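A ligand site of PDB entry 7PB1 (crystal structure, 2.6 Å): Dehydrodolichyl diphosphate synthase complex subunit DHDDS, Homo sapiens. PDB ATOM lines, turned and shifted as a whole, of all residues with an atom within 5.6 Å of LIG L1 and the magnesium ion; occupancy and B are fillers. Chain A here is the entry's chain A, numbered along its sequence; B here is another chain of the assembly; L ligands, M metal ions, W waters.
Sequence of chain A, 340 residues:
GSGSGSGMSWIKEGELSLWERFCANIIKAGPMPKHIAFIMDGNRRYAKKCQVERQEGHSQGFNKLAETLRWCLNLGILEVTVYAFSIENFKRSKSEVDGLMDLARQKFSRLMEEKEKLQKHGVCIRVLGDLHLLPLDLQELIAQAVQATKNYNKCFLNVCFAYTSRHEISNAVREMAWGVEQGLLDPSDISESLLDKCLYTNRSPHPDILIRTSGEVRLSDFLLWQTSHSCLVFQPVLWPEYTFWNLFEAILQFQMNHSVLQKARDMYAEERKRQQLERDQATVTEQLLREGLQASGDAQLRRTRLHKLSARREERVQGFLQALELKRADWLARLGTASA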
ATOM      1  N   ILE A  39       8.552  -8.189  27.066  1.00  0.00           N
ATOM      2  CA  ILE A  39       9.839  -7.492  27.073  1.00  0.00           C
ATOM      3  C   ILE A  39       9.505  -6.032  27.342  1.00  0.00           C
ATOM      4  O   ILE A  39       9.176  -5.270  26.428  1.00  0.00           O
ATOM      5  CB  ILE A  39      10.607  -7.672  25.764  1.00  0.00           C
ATOM      6  CG1 ILE A  39      11.030  -9.118  25.591  1.00  0.00           C
ATOM      7  CG2 ILE A  39      11.840  -6.767  25.739  1.00  0.00           C
ATOM      8  CD1 ILE A  39      11.502  -9.406  24.219  1.00  0.00           C
ATOM      9  N   MET A  40       9.588  -5.644  28.609  1.00  0.00           N
ATOM     10  CA  MET A  40       9.244  -4.296  29.023  1.00  0.00           C
ATOM     11  C   MET A  40      10.324  -3.319  28.566  1.00  0.00           C
ATOM     12  O   MET A  40      11.276  -3.035  29.289  1.00  0.00           O
ATOM     13  CB  MET A  40       9.076  -4.239  30.543  1.00  0.00           C
ATOM     14  CG  MET A  40       8.298  -5.427  31.091  1.00  0.00           C
ATOM     15  SD  MET A  40       8.089  -5.429  32.890  1.00  0.00           S
ATOM     16  CE  MET A  40       9.766  -5.710  33.434  1.00  0.00           C
ATOM     17  N   ASP A  41      10.171  -2.805  27.351  1.00  0.00           N
ATOM     18  CA  ASP A  41      11.195  -1.987  26.710  1.00  0.00           C
ATOM     19  C   ASP A  41      10.682  -0.568  26.500  1.00  0.00           C
ATOM     20  O   ASP A  41       9.475  -0.354  26.330  1.00  0.00           O
ATOM     21  CB  ASP A  41      11.602  -2.617  25.370  1.00  0.00           C
ATOM     22  CG  ASP A  41      12.968  -2.182  24.920  1.00  0.00           C
ATOM     23  OD1 ASP A  41      13.763  -1.782  25.799  1.00  0.00           O
ATOM     24  OD2 ASP A  41      13.247  -2.249  23.704  1.00  0.00           O
ATOM     25  N   GLY A  42      11.595   0.398  26.535  1.00  0.00           N
ATOM     26  CA  GLY A  42      11.262   1.789  26.314  1.00  0.00           C
ATOM     27  C   GLY A  42      11.252   2.679  27.549  1.00  0.00           C
ATOM     28  O   GLY A  42      10.875   3.847  27.438  1.00  0.00           O
ATOM     29  N   ARG A  44      13.605   4.194  29.262  1.00  0.00           N
ATOM     30  CA  ARG A  44      14.442   5.392  29.208  1.00  0.00           C
ATOM     31  C   ARG A  44      13.905   6.404  28.202  1.00  0.00           C
ATOM     32  O   ARG A  44      13.932   7.618  28.459  1.00  0.00           O
ATOM     33  CB  ARG A  44      15.873   5.018  28.875  1.00  0.00           C
ATOM     34  CG  ARG A  44      16.604   4.323  30.007  1.00  0.00           C
ATOM     35  CD  ARG A  44      17.500   3.248  29.455  1.00  0.00           C
ATOM     36  NE  ARG A  44      18.817   3.740  29.070  1.00  0.00           N
ATOM     37  CZ  ARG A  44      19.668   3.072  28.314  1.00  0.00           C
ATOM     38  NH1 ARG A  44      19.336   1.879  27.844  1.00  0.00           N
ATOM     39  NH2 ARG A  44      20.846   3.592  28.007  1.00  0.00           N
ATOM     40  N   ARG A  45      13.439   5.929  27.047  1.00  0.00           N
ATOM     41  CA  ARG A  45      12.890   6.847  26.057  1.00  0.00           C
ATOM     42  C   ARG A  45      11.677   7.579  26.622  1.00  0.00           C
ATOM     43  O   ARG A  45      11.518   8.793  26.418  1.00  0.00           O
ATOM     44  CB  ARG A  45      12.513   6.091  24.787  1.00  0.00           C
ATOM     45  CG  ARG A  45      13.670   5.857  23.840  1.00  0.00           C
ATOM     46  CD  ARG A  45      13.320   4.783  22.842  1.00  0.00           C
ATOM     47  NE  ARG A  45      13.488   3.436  23.380  1.00  0.00           N
ATOM     48  CZ  ARG A  45      13.135   2.337  22.724  1.00  0.00           C
ATOM     49  NH1 ARG A  45      12.590   2.426  21.516  1.00  0.00           N
ATOM     50  NH2 ARG A  45      13.323   1.140  23.274  1.00  0.00           N
ATOM     51  N   TYR A  83      10.722  -9.776  31.208  1.00  0.00           N
ATOM     52  CA  TYR A  83      12.162  -9.541  31.075  1.00  0.00           C
ATOM     53  C   TYR A  83      12.500  -8.302  31.888  1.00  0.00           C
ATOM     54  O   TYR A  83      12.227  -7.173  31.466  1.00  0.00           O
ATOM     55  CB  TYR A  83      12.520  -9.375  29.605  1.00  0.00           C
ATOM     56  CG  TYR A  83      13.931  -9.771  29.239  1.00  0.00           C
ATOM     57  CD1 TYR A  83      14.308  -9.881  27.905  1.00  0.00           C
ATOM     58  CD2 TYR A  83      14.895 -10.007  30.212  1.00  0.00           C
ATOM     59  CE1 TYR A  83      15.586 -10.230  27.549  1.00  0.00           C
ATOM     60  CE2 TYR A  83      16.186 -10.350  29.856  1.00  0.00           C
ATOM     61  CZ  TYR A  83      16.522 -10.459  28.525  1.00  0.00           C
ATOM     62  OH  TYR A  83      17.804 -10.816  28.137  1.00  0.00           O
ATOM     63  N   ALA A  84      13.093  -8.505  33.062  1.00  0.00           N
ATOM     64  CA  ALA A  84      13.334  -7.425  34.010  1.00  0.00           C
ATOM     65  C   ALA A  84      14.761  -6.898  33.987  1.00  0.00           C
ATOM     66  O   ALA A  84      14.969  -5.715  34.253  1.00  0.00           O
ATOM     67  CB  ALA A  84      12.998  -7.883  35.431  1.00  0.00           C
ATOM     68  N   PHE A  85      15.751  -7.754  33.707  1.00  0.00           N
ATOM     69  CA  PHE A  85      17.126  -7.280  33.639  1.00  0.00           C
ATOM     70  C   PHE A  85      17.957  -8.296  32.869  1.00  0.00           C
ATOM     71  O   PHE A  85      18.079  -9.447  33.300  1.00  0.00           O
ATOM     72  CB  PHE A  85      17.711  -7.070  35.034  1.00  0.00           C
ATOM     73  CG  PHE A  85      18.953  -6.224  35.039  1.00  0.00           C
ATOM     74  CD1 PHE A  85      20.210  -6.821  35.001  1.00  0.00           C
ATOM     75  CD2 PHE A  85      18.868  -4.841  35.059  1.00  0.00           C
ATOM     76  CE1 PHE A  85      21.360  -6.041  34.993  1.00  0.00           C
ATOM     77  CE2 PHE A  85      20.007  -4.069  35.052  1.00  0.00           C
ATOM     78  CZ  PHE A  85      21.254  -4.665  35.024  1.00  0.00           C
ATOM     79  N   SER A  86      18.548  -7.857  31.757  1.00  0.00           N
ATOM     80  CA  SER A  86      19.382  -8.708  30.922  1.00  0.00           C
ATOM     81  C   SER A  86      20.821  -8.703  31.393  1.00  0.00           C
ATOM     82  O   SER A  86      21.329  -7.703  31.917  1.00  0.00           O
ATOM     83  CB  SER A  86      19.335  -8.263  29.463  1.00  0.00           C
ATOM     84  OG  SER A  86      20.236  -9.047  28.694  1.00  0.00           O
ATOM     85  N   ASN A  89      22.516  -5.827  30.040  1.00  0.00           N
ATOM     86  CA  ASN A  89      22.336  -4.551  30.723  1.00  0.00           C
ATOM     87  C   ASN A  89      23.413  -4.273  31.769  1.00  0.00           C
ATOM     88  O   ASN A  89      23.510  -3.140  32.241  1.00  0.00           O
ATOM     89  CB  ASN A  89      20.957  -4.497  31.376  1.00  0.00           C
ATOM     90  CG  ASN A  89      19.837  -4.643  30.375  1.00  0.00           C
ATOM     91  OD1 ASN A  89      18.861  -5.358  30.622  1.00  0.00           O
ATOM     92  ND2 ASN A  89      19.950  -3.954  29.247  1.00  0.00           N
ATOM     93  N   ARG A  92      25.665  -1.135  31.111  1.00  0.00           N
ATOM     94  CA  ARG A  92      25.225   0.240  31.223  1.00  0.00           C
ATOM     95  C   ARG A  92      26.075   0.969  32.262  1.00  0.00           C
ATOM     96  O   ARG A  92      26.984   0.391  32.868  1.00  0.00           O
ATOM     97  CB  ARG A  92      23.736   0.303  31.572  1.00  0.00           C
ATOM     98  CG  ARG A  92      22.857  -0.433  30.565  1.00  0.00           C
ATOM     99  CD  ARG A  92      21.388  -0.090  30.673  1.00  0.00           C
ATOM    100  NE  ARG A  92      20.617  -0.758  29.637  1.00  0.00           N
ATOM    101  CZ  ARG A  92      19.299  -0.650  29.469  1.00  0.00           C
ATOM    102  NH1 ARG A  92      18.575   0.109  30.290  1.00  0.00           N
ATOM    103  NH2 ARG A  92      18.694  -1.310  28.490  1.00  0.00           N
ATOM    104  N   ARG A 212       6.862  -7.340  22.892  1.00  0.00           N
ATOM    105  CA  ARG A 212       7.930  -6.361  23.047  1.00  0.00           C
ATOM    106  C   ARG A 212       7.391  -4.982  22.721  1.00  0.00           C
ATOM    107  O   ARG A 212       6.760  -4.787  21.671  1.00  0.00           O
ATOM    108  CB  ARG A 212       9.143  -6.652  22.167  1.00  0.00           C
ATOM    109  CG  ARG A 212      10.176  -5.527  22.247  1.00  0.00           C
ATOM    110  CD  ARG A 212      11.559  -6.001  21.973  1.00  0.00           C
ATOM    111  NE  ARG A 212      12.571  -5.097  22.486  1.00  0.00           N
ATOM    112  CZ  ARG A 212      13.883  -5.322  22.371  1.00  0.00           C
ATOM    113  NH1 ARG A 212      14.308  -6.414  21.757  1.00  0.00           N
ATOM    114  NH2 ARG A 212      14.757  -4.462  22.870  1.00  0.00           N
ATOM    115  N   GLU A 216      10.914  -1.611  18.638  1.00  0.00           N
ATOM    116  CA  GLU A 216      11.910  -2.605  18.284  1.00  0.00           C
ATOM    117  C   GLU A 216      11.257  -3.877  17.749  1.00  0.00           C
ATOM    118  O   GLU A 216      10.267  -4.358  18.299  1.00  0.00           O
ATOM    119  CB  GLU A 216      12.782  -2.921  19.496  1.00  0.00           C
ATOM    120  CG  GLU A 216      13.327  -1.660  20.182  1.00  0.00           C
ATOM    121  CD  GLU A 216      13.822  -0.613  19.189  1.00  0.00           C
ATOM    122  OE1 GLU A 216      14.595  -0.975  18.276  1.00  0.00           O
ATOM    123  OE2 GLU A 216      13.417   0.573  19.307  1.00  0.00           O
ATOM    124  N   ARG A 218      12.981  -6.833  17.465  1.00  0.00           N
ATOM    125  CA  ARG A 218      13.930  -7.877  17.799  1.00  0.00           C
ATOM    126  C   ARG A 218      13.547  -8.481  19.149  1.00  0.00           C
ATOM    127  O   ARG A 218      12.763  -7.915  19.902  1.00  0.00           O
ATOM    128  CB  ARG A 218      15.360  -7.329  17.840  1.00  0.00           C
ATOM    129  CG  ARG A 218      15.507  -6.041  18.607  1.00  0.00           C
ATOM    130  CD  ARG A 218      16.962  -5.693  18.755  1.00  0.00           C
ATOM    131  NE  ARG A 218      17.114  -4.443  19.485  1.00  0.00           N
ATOM    132  CZ  ARG A 218      17.111  -3.243  18.918  1.00  0.00           C
ATOM    133  NH1 ARG A 218      16.974  -3.139  17.605  1.00  0.00           N
ATOM    134  NH2 ARG A 218      17.254  -2.162  19.672  1.00  0.00           N
ATOM    135  N   SER A 220      15.978  -9.601  21.441  1.00  0.00           N
ATOM    136  CA  SER A 220      17.037  -9.307  22.400  1.00  0.00           C
ATOM    137  C   SER A 220      17.198 -10.416  23.435  1.00  0.00           C
ATOM    138  O   SER A 220      17.034 -10.223  24.641  1.00  0.00           O
ATOM    139  CB  SER A 220      16.782  -7.959  23.091  1.00  0.00           C
ATOM    140  OG  SER A 220      16.909  -6.882  22.167  1.00  0.00           O
ATOM    141  N   LEU B 186      19.370 -11.330  18.226  1.00  0.00           N
ATOM    142  CA  LEU B 186      19.362  -9.908  17.961  1.00  0.00           C
ATOM    143  C   LEU B 186      18.809  -9.564  16.582  1.00  0.00           C
ATOM    144  O   LEU B 186      18.771  -8.373  16.230  1.00  0.00           O
ATOM    145  CB  LEU B 186      20.775  -9.331  18.130  1.00  0.00           C
ATOM    146  CG  LEU B 186      21.187  -9.135  19.590  1.00  0.00           C
ATOM    147  CD1 LEU B 186      22.653  -8.762  19.691  1.00  0.00           C
ATOM    148  CD2 LEU B 186      20.336  -8.053  20.230  1.00  0.00           C
ATOM    149  N   GLU B 214      17.997   0.828  15.098  1.00  0.00           N
ATOM    150  CA  GLU B 214      19.049   1.135  16.060  1.00  0.00           C
ATOM    151  C   GLU B 214      19.233  -0.069  16.976  1.00  0.00           C
ATOM    152  O   GLU B 214      18.370  -0.361  17.800  1.00  0.00           O
ATOM    153  CB  GLU B 214      18.714   2.397  16.856  1.00  0.00           C
ATOM    154  N   GLN B 215      20.352  -0.767  16.811  1.00  0.00           N
ATOM    155  CA  GLN B 215      20.682  -1.900  17.674  1.00  0.00           C
ATOM    156  C   GLN B 215      21.477  -1.375  18.858  1.00  0.00           C
ATOM    157  O   GLN B 215      22.649  -1.013  18.729  1.00  0.00           O
ATOM    158  CB  GLN B 215      21.468  -2.966  16.900  1.00  0.00           C
ATOM    159  CG  GLN B 215      21.065  -3.123  15.435  1.00  0.00           C
ATOM    160  N   ARG B 216      20.834  -1.326  20.033  1.00  0.00           N
ATOM    161  CA  ARG B 216      21.512  -0.809  21.216  1.00  0.00           C
ATOM    162  C   ARG B 216      22.333  -1.859  21.926  1.00  0.00           C
ATOM    163  O   ARG B 216      23.263  -1.508  22.662  1.00  0.00           O
ATOM    164  CB  ARG B 216      20.485  -0.205  22.181  1.00  0.00           C
ATOM    165  CG  ARG B 216      20.171   1.252  21.898  1.00  0.00           C
ATOM    166  CD  ARG B 216      19.025   1.766  22.767  1.00  0.00           C
ATOM    167  NE  ARG B 216      17.761   1.101  22.479  1.00  0.00           N
ATOM    168  CZ  ARG B 216      17.016   1.352  21.407  1.00  0.00           C
ATOM    169  NH1 ARG B 216      17.414   2.255  20.511  1.00  0.00           N
ATOM    170  NH2 ARG B 216      15.881   0.688  21.229  1.00  0.00           N
ATOM    171  N   LEU B 217      22.013  -3.145  21.724  1.00  0.00           N
ATOM    172  CA  LEU B 217      22.808  -4.248  22.265  1.00  0.00           C
ATOM    173  C   LEU B 217      22.894  -4.178  23.785  1.00  0.00           C
ATOM    174  O   LEU B 217      23.947  -4.439  24.379  1.00  0.00           O
ATOM    175  CB  LEU B 217      24.203  -4.289  21.634  1.00  0.00           C
ATOM    176  N   GLY B 218      21.784  -3.811  24.434  1.00  0.00           N
ATOM    177  CA  GLY B 218      21.700  -3.830  25.873  1.00  0.00           C
ATOM    178  C   GLY B 218      22.257  -2.616  26.580  1.00  0.00           C
ATOM    179  O   GLY B 218      21.920  -2.391  27.756  1.00  0.00           O
ATOM    180  N   LYS B 219      23.114  -1.833  25.928  1.00  0.00           N
ATOM    181  CA  LYS B 219      23.677  -0.631  26.552  1.00  0.00           C
ATOM    182  C   LYS B 219      22.677   0.513  26.504  1.00  0.00           C
ATOM    183  O   LYS B 219      22.927   1.609  27.016  1.00  0.00           O
ATOM    184  CB  LYS B 219      24.994  -0.222  25.858  1.00  0.00           C
ATOM    185  CG  LYS B 219      26.247  -0.633  26.603  1.00  0.00           C
ATOM    186  CD  LYS B 219      27.524  -0.326  25.815  1.00  0.00           C
ATOM    187  OXT LYS B 219      21.577   0.373  25.950  1.00  0.00           O
HETATM  188  P1  LIG L   1      18.268  -3.690  23.074  1.00  0.00           P
HETATM  189  O1  LIG L   1      16.980  -3.965  24.031  1.00  0.00           O
HETATM  190  P2  LIG L   1      17.077  -3.703  25.652  1.00  0.00           P
HETATM  191  O2  LIG L   1      18.632  -4.944  22.317  1.00  0.00           O
HETATM  192  O3  LIG L   1      17.926  -2.563  22.129  1.00  0.00           O
HETATM  193  O4  LIG L   1      19.393  -3.239  23.982  1.00  0.00           O
HETATM  194  O5  LIG L   1      16.820  -2.249  25.964  1.00  0.00           O
HETATM  195  O6  LIG L   1      18.434  -4.122  26.173  1.00  0.00           O
HETATM  196  S1  LIG L   1      15.611  -4.932  26.520  1.00  0.00           S
HETATM  197  C1  LIG L   1      16.576  -5.936  27.672  1.00  0.00           C
HETATM  198  C2  LIG L   1      15.633  -6.867  28.430  1.00  0.00           C
HETATM  199  C3  LIG L   1      14.867  -6.051  29.457  1.00  0.00           C
HETATM  200  C4  LIG L   1      13.490  -5.483  29.115  1.00  0.00           C
HETATM  201  C5  LIG L   1      15.412  -5.842  30.632  1.00  0.00           C
HETATM  202  C1  LG2 L   2       7.485  -7.617  41.234  1.00  0.00           C
HETATM  203  C2  LG2 L   2       8.502 -10.012  41.585  1.00  0.00           C
HETATM  204  C3  LG2 L   2       8.687  -8.544  41.198  1.00  0.00           C
HETATM  205  C4  LG2 L   2       9.906  -8.123  40.840  1.00  0.00           C
HETATM  206  C5  LG2 L   2      10.153  -6.649  40.438  1.00  0.00           C
HETATM  207  C6  LG2 L   2      12.681  -5.072  40.060  1.00  0.00           C
HETATM  208  C7  LG2 L   2      11.649  -5.313  38.964  1.00  0.00           C
HETATM  209  C8  LG2 L   2      10.783  -6.588  39.028  1.00  0.00           C
HETATM  210  C9  LG2 L   2      11.511  -4.386  37.989  1.00  0.00           C
HETATM  211  C10 LG2 L   2      10.483  -4.536  36.827  1.00  0.00           C
HETATM  212  C11 LG2 L   2      10.206  -3.141  36.164  1.00  0.00           C
HETATM  213  C12 LG2 L   2      11.466  -2.576  35.440  1.00  0.00           C
HETATM  214  C13 LG2 L   2      12.511  -1.745  36.183  1.00  0.00           C
HETATM  215  C14 LG2 L   2      11.664  -2.787  34.137  1.00  0.00           C
HETATM  216  C15 LG2 L   2      12.941  -2.196  33.497  1.00  0.00           C
HETATM  217  C16 LG2 L   2      13.827  -3.323  32.886  1.00  0.00           C
HETATM  218  C17 LG2 L   2      14.562  -2.792  31.655  1.00  0.00           C
HETATM  219  C18 LG2 L   2      16.087  -2.721  31.620  1.00  0.00           C
HETATM  220  C19 LG2 L   2      13.803  -2.375  30.622  1.00  0.00           C
HETATM  221  C20 LG2 L   2      14.376  -1.831  29.316  1.00  0.00           C
HETATM  222  O1  LG2 L   2      13.852  -0.564  29.011  1.00  0.00           O
HETATM  223  P1  LG2 L   2      15.081   0.480  28.602  1.00  0.00           P
HETATM  224  O2  LG2 L   2      15.823   0.842  29.866  1.00  0.00           O
HETATM  225  O3  LG2 L   2      14.452   1.805  27.858  1.00  0.00           O
HETATM  226  O4  LG2 L   2      16.066  -0.180  27.672  1.00  0.00           O
HETATM  227  P2  LG2 L   2      14.982   2.239  26.376  1.00  0.00           P
HETATM  228  O5  LG2 L   2      14.272   3.492  25.943  1.00  0.00           O
HETATM  229  O6  LG2 L   2      16.476   2.450  26.458  1.00  0.00           O
HETATM  230  O7  LG2 L   2      14.670   1.141  25.400  1.00  0.00           O
HETATM  231 MG    MG M   1      15.526  -0.562  25.614  1.00  0.00          MG
HETATM  232  O   HOH W   1      17.172   0.296  24.872  1.00  0.00           O
HETATM  233  O   HOH W   2      15.629  -1.270  23.556  1.00  0.00           O
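Residues that only touch LIG L1: Ile 39 (3.97 Å), Met 40 (3.3 Å), Tyr 83 (3.2 Å), Ala 84 (3.6 Å), Phe 85 (3.6 Å) and Ser 86 (3.9 Å). Of the 23 residues printed, 15 come within 4 Å of LIG L1.
O3 of LG2 L2 sits close to N of Gly 42, at 3.4 Å. The backbone NH of Leu 217 of chain B sits at hydrogen-bond distance from an oxygen (O4) of LIG L1 (3.5 Å). ND2 of Asn 89 lies within hydrogen-bond range of O6 of LIG L1. An oxygen (O3) of LIG L1 is in salt-bridge range of the guanidinium group of Arg 218 of chain A (2.6 Å). An oxygen (O6) of LG2 L2 lies within salt-bridge range of the guanidinium group of Arg 44, at 3.2 Å. O3 of LIG L1 lies within salt-bridge range of NE of Arg 216 of chain B, at 3.7 Å. The side-chain hydroxyl (OG) of Ser 220 lies within hydrogen-bond range of an oxygen (O2) of LIG L1, at 2.6 Å. The guanidinium group (NH1) of Arg 92 is in salt-bridge range of an oxygen (O2) of LG2 L2, 2.9 Å away. N of Arg 45 lies within hydrogen-bond range of O5 of LG2 L2 (2.8 Å). O4 of LIG L1 is in hydrogen-bond range of N of Gly 218 of chain B, at 2.5 Å. The backbone NH of Arg 44 is in hydrogen-bond range of an oxygen (O3) of LG2 L2, at 2.9 Å. NH2 of Arg 212 lies within salt-bridge range of O3 of LIG L1 (3.8 Å). The guanidinium group of Arg 92 is in salt-bridge range of an oxygen (O6) of LIG L1, 3.7 Å away. An oxygen (O5) of LG2 L2 is in salt-bridge range of the guanidinium group (NE) of Arg 45 (2.7 Å).
Water W1 lies within hydrogen-bond range of the guanidinium group of Arg 216 of chain B (2.6 Å) and an oxygen (O6) of LG2 L2 (2.8 Å).
NH1 of Arg 45 is in salt-bridge range of OE2 of Glu 216 of chain A. The side-chain carboxylate (OE1) of Glu 216 of chain A is in salt-bridge range of the guanidinium group (NH2) of Arg 218 of chain A, 3.2 Å away. The guanidinium group (NH1) of Arg 212 sits at hydrogen-bond distance from the backbone carbonyl oxygen (O) of Arg 218 of chain A (2.8 Å). The guanidinium group of Arg 216 of chain B lies within salt-bridge range of the side-chain carboxylate of Glu 216 of chain A (3.1 Å). The side-chain hydroxyl (OH) of Tyr 83 is in hydrogen-bond range of the side-chain hydroxyl (OG) of Ser 86. The side-chain carboxylate (OD2) of Asp 41 lies within salt-bridge range of the guanidinium group (NH2) of Arg 45 (3.4 Å). NH2 of Arg 92 lies close to ND2 of Asn 89 (3.0 Å). The side-chain amide nitrogen of Asn 89 is in hydrogen-bond range of the backbone carbonyl oxygen of Gly 218 of chain B (2.9 Å).
The magnesium ion is bound by O7 of LG2 L2 (1.9 Å), water W1 (2.0 Å), OD1 of Asp 41 (2.2 Å), O5 of LIG L1 (2.2 Å), O4 of LG2 L2 (2.2 Å) and water W2 (2.2 Å).
Arg 45 touches the magnesium ion. Two residues have an atom within 4 Å of the magnesium ion: Asp 41 and Arg 45.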
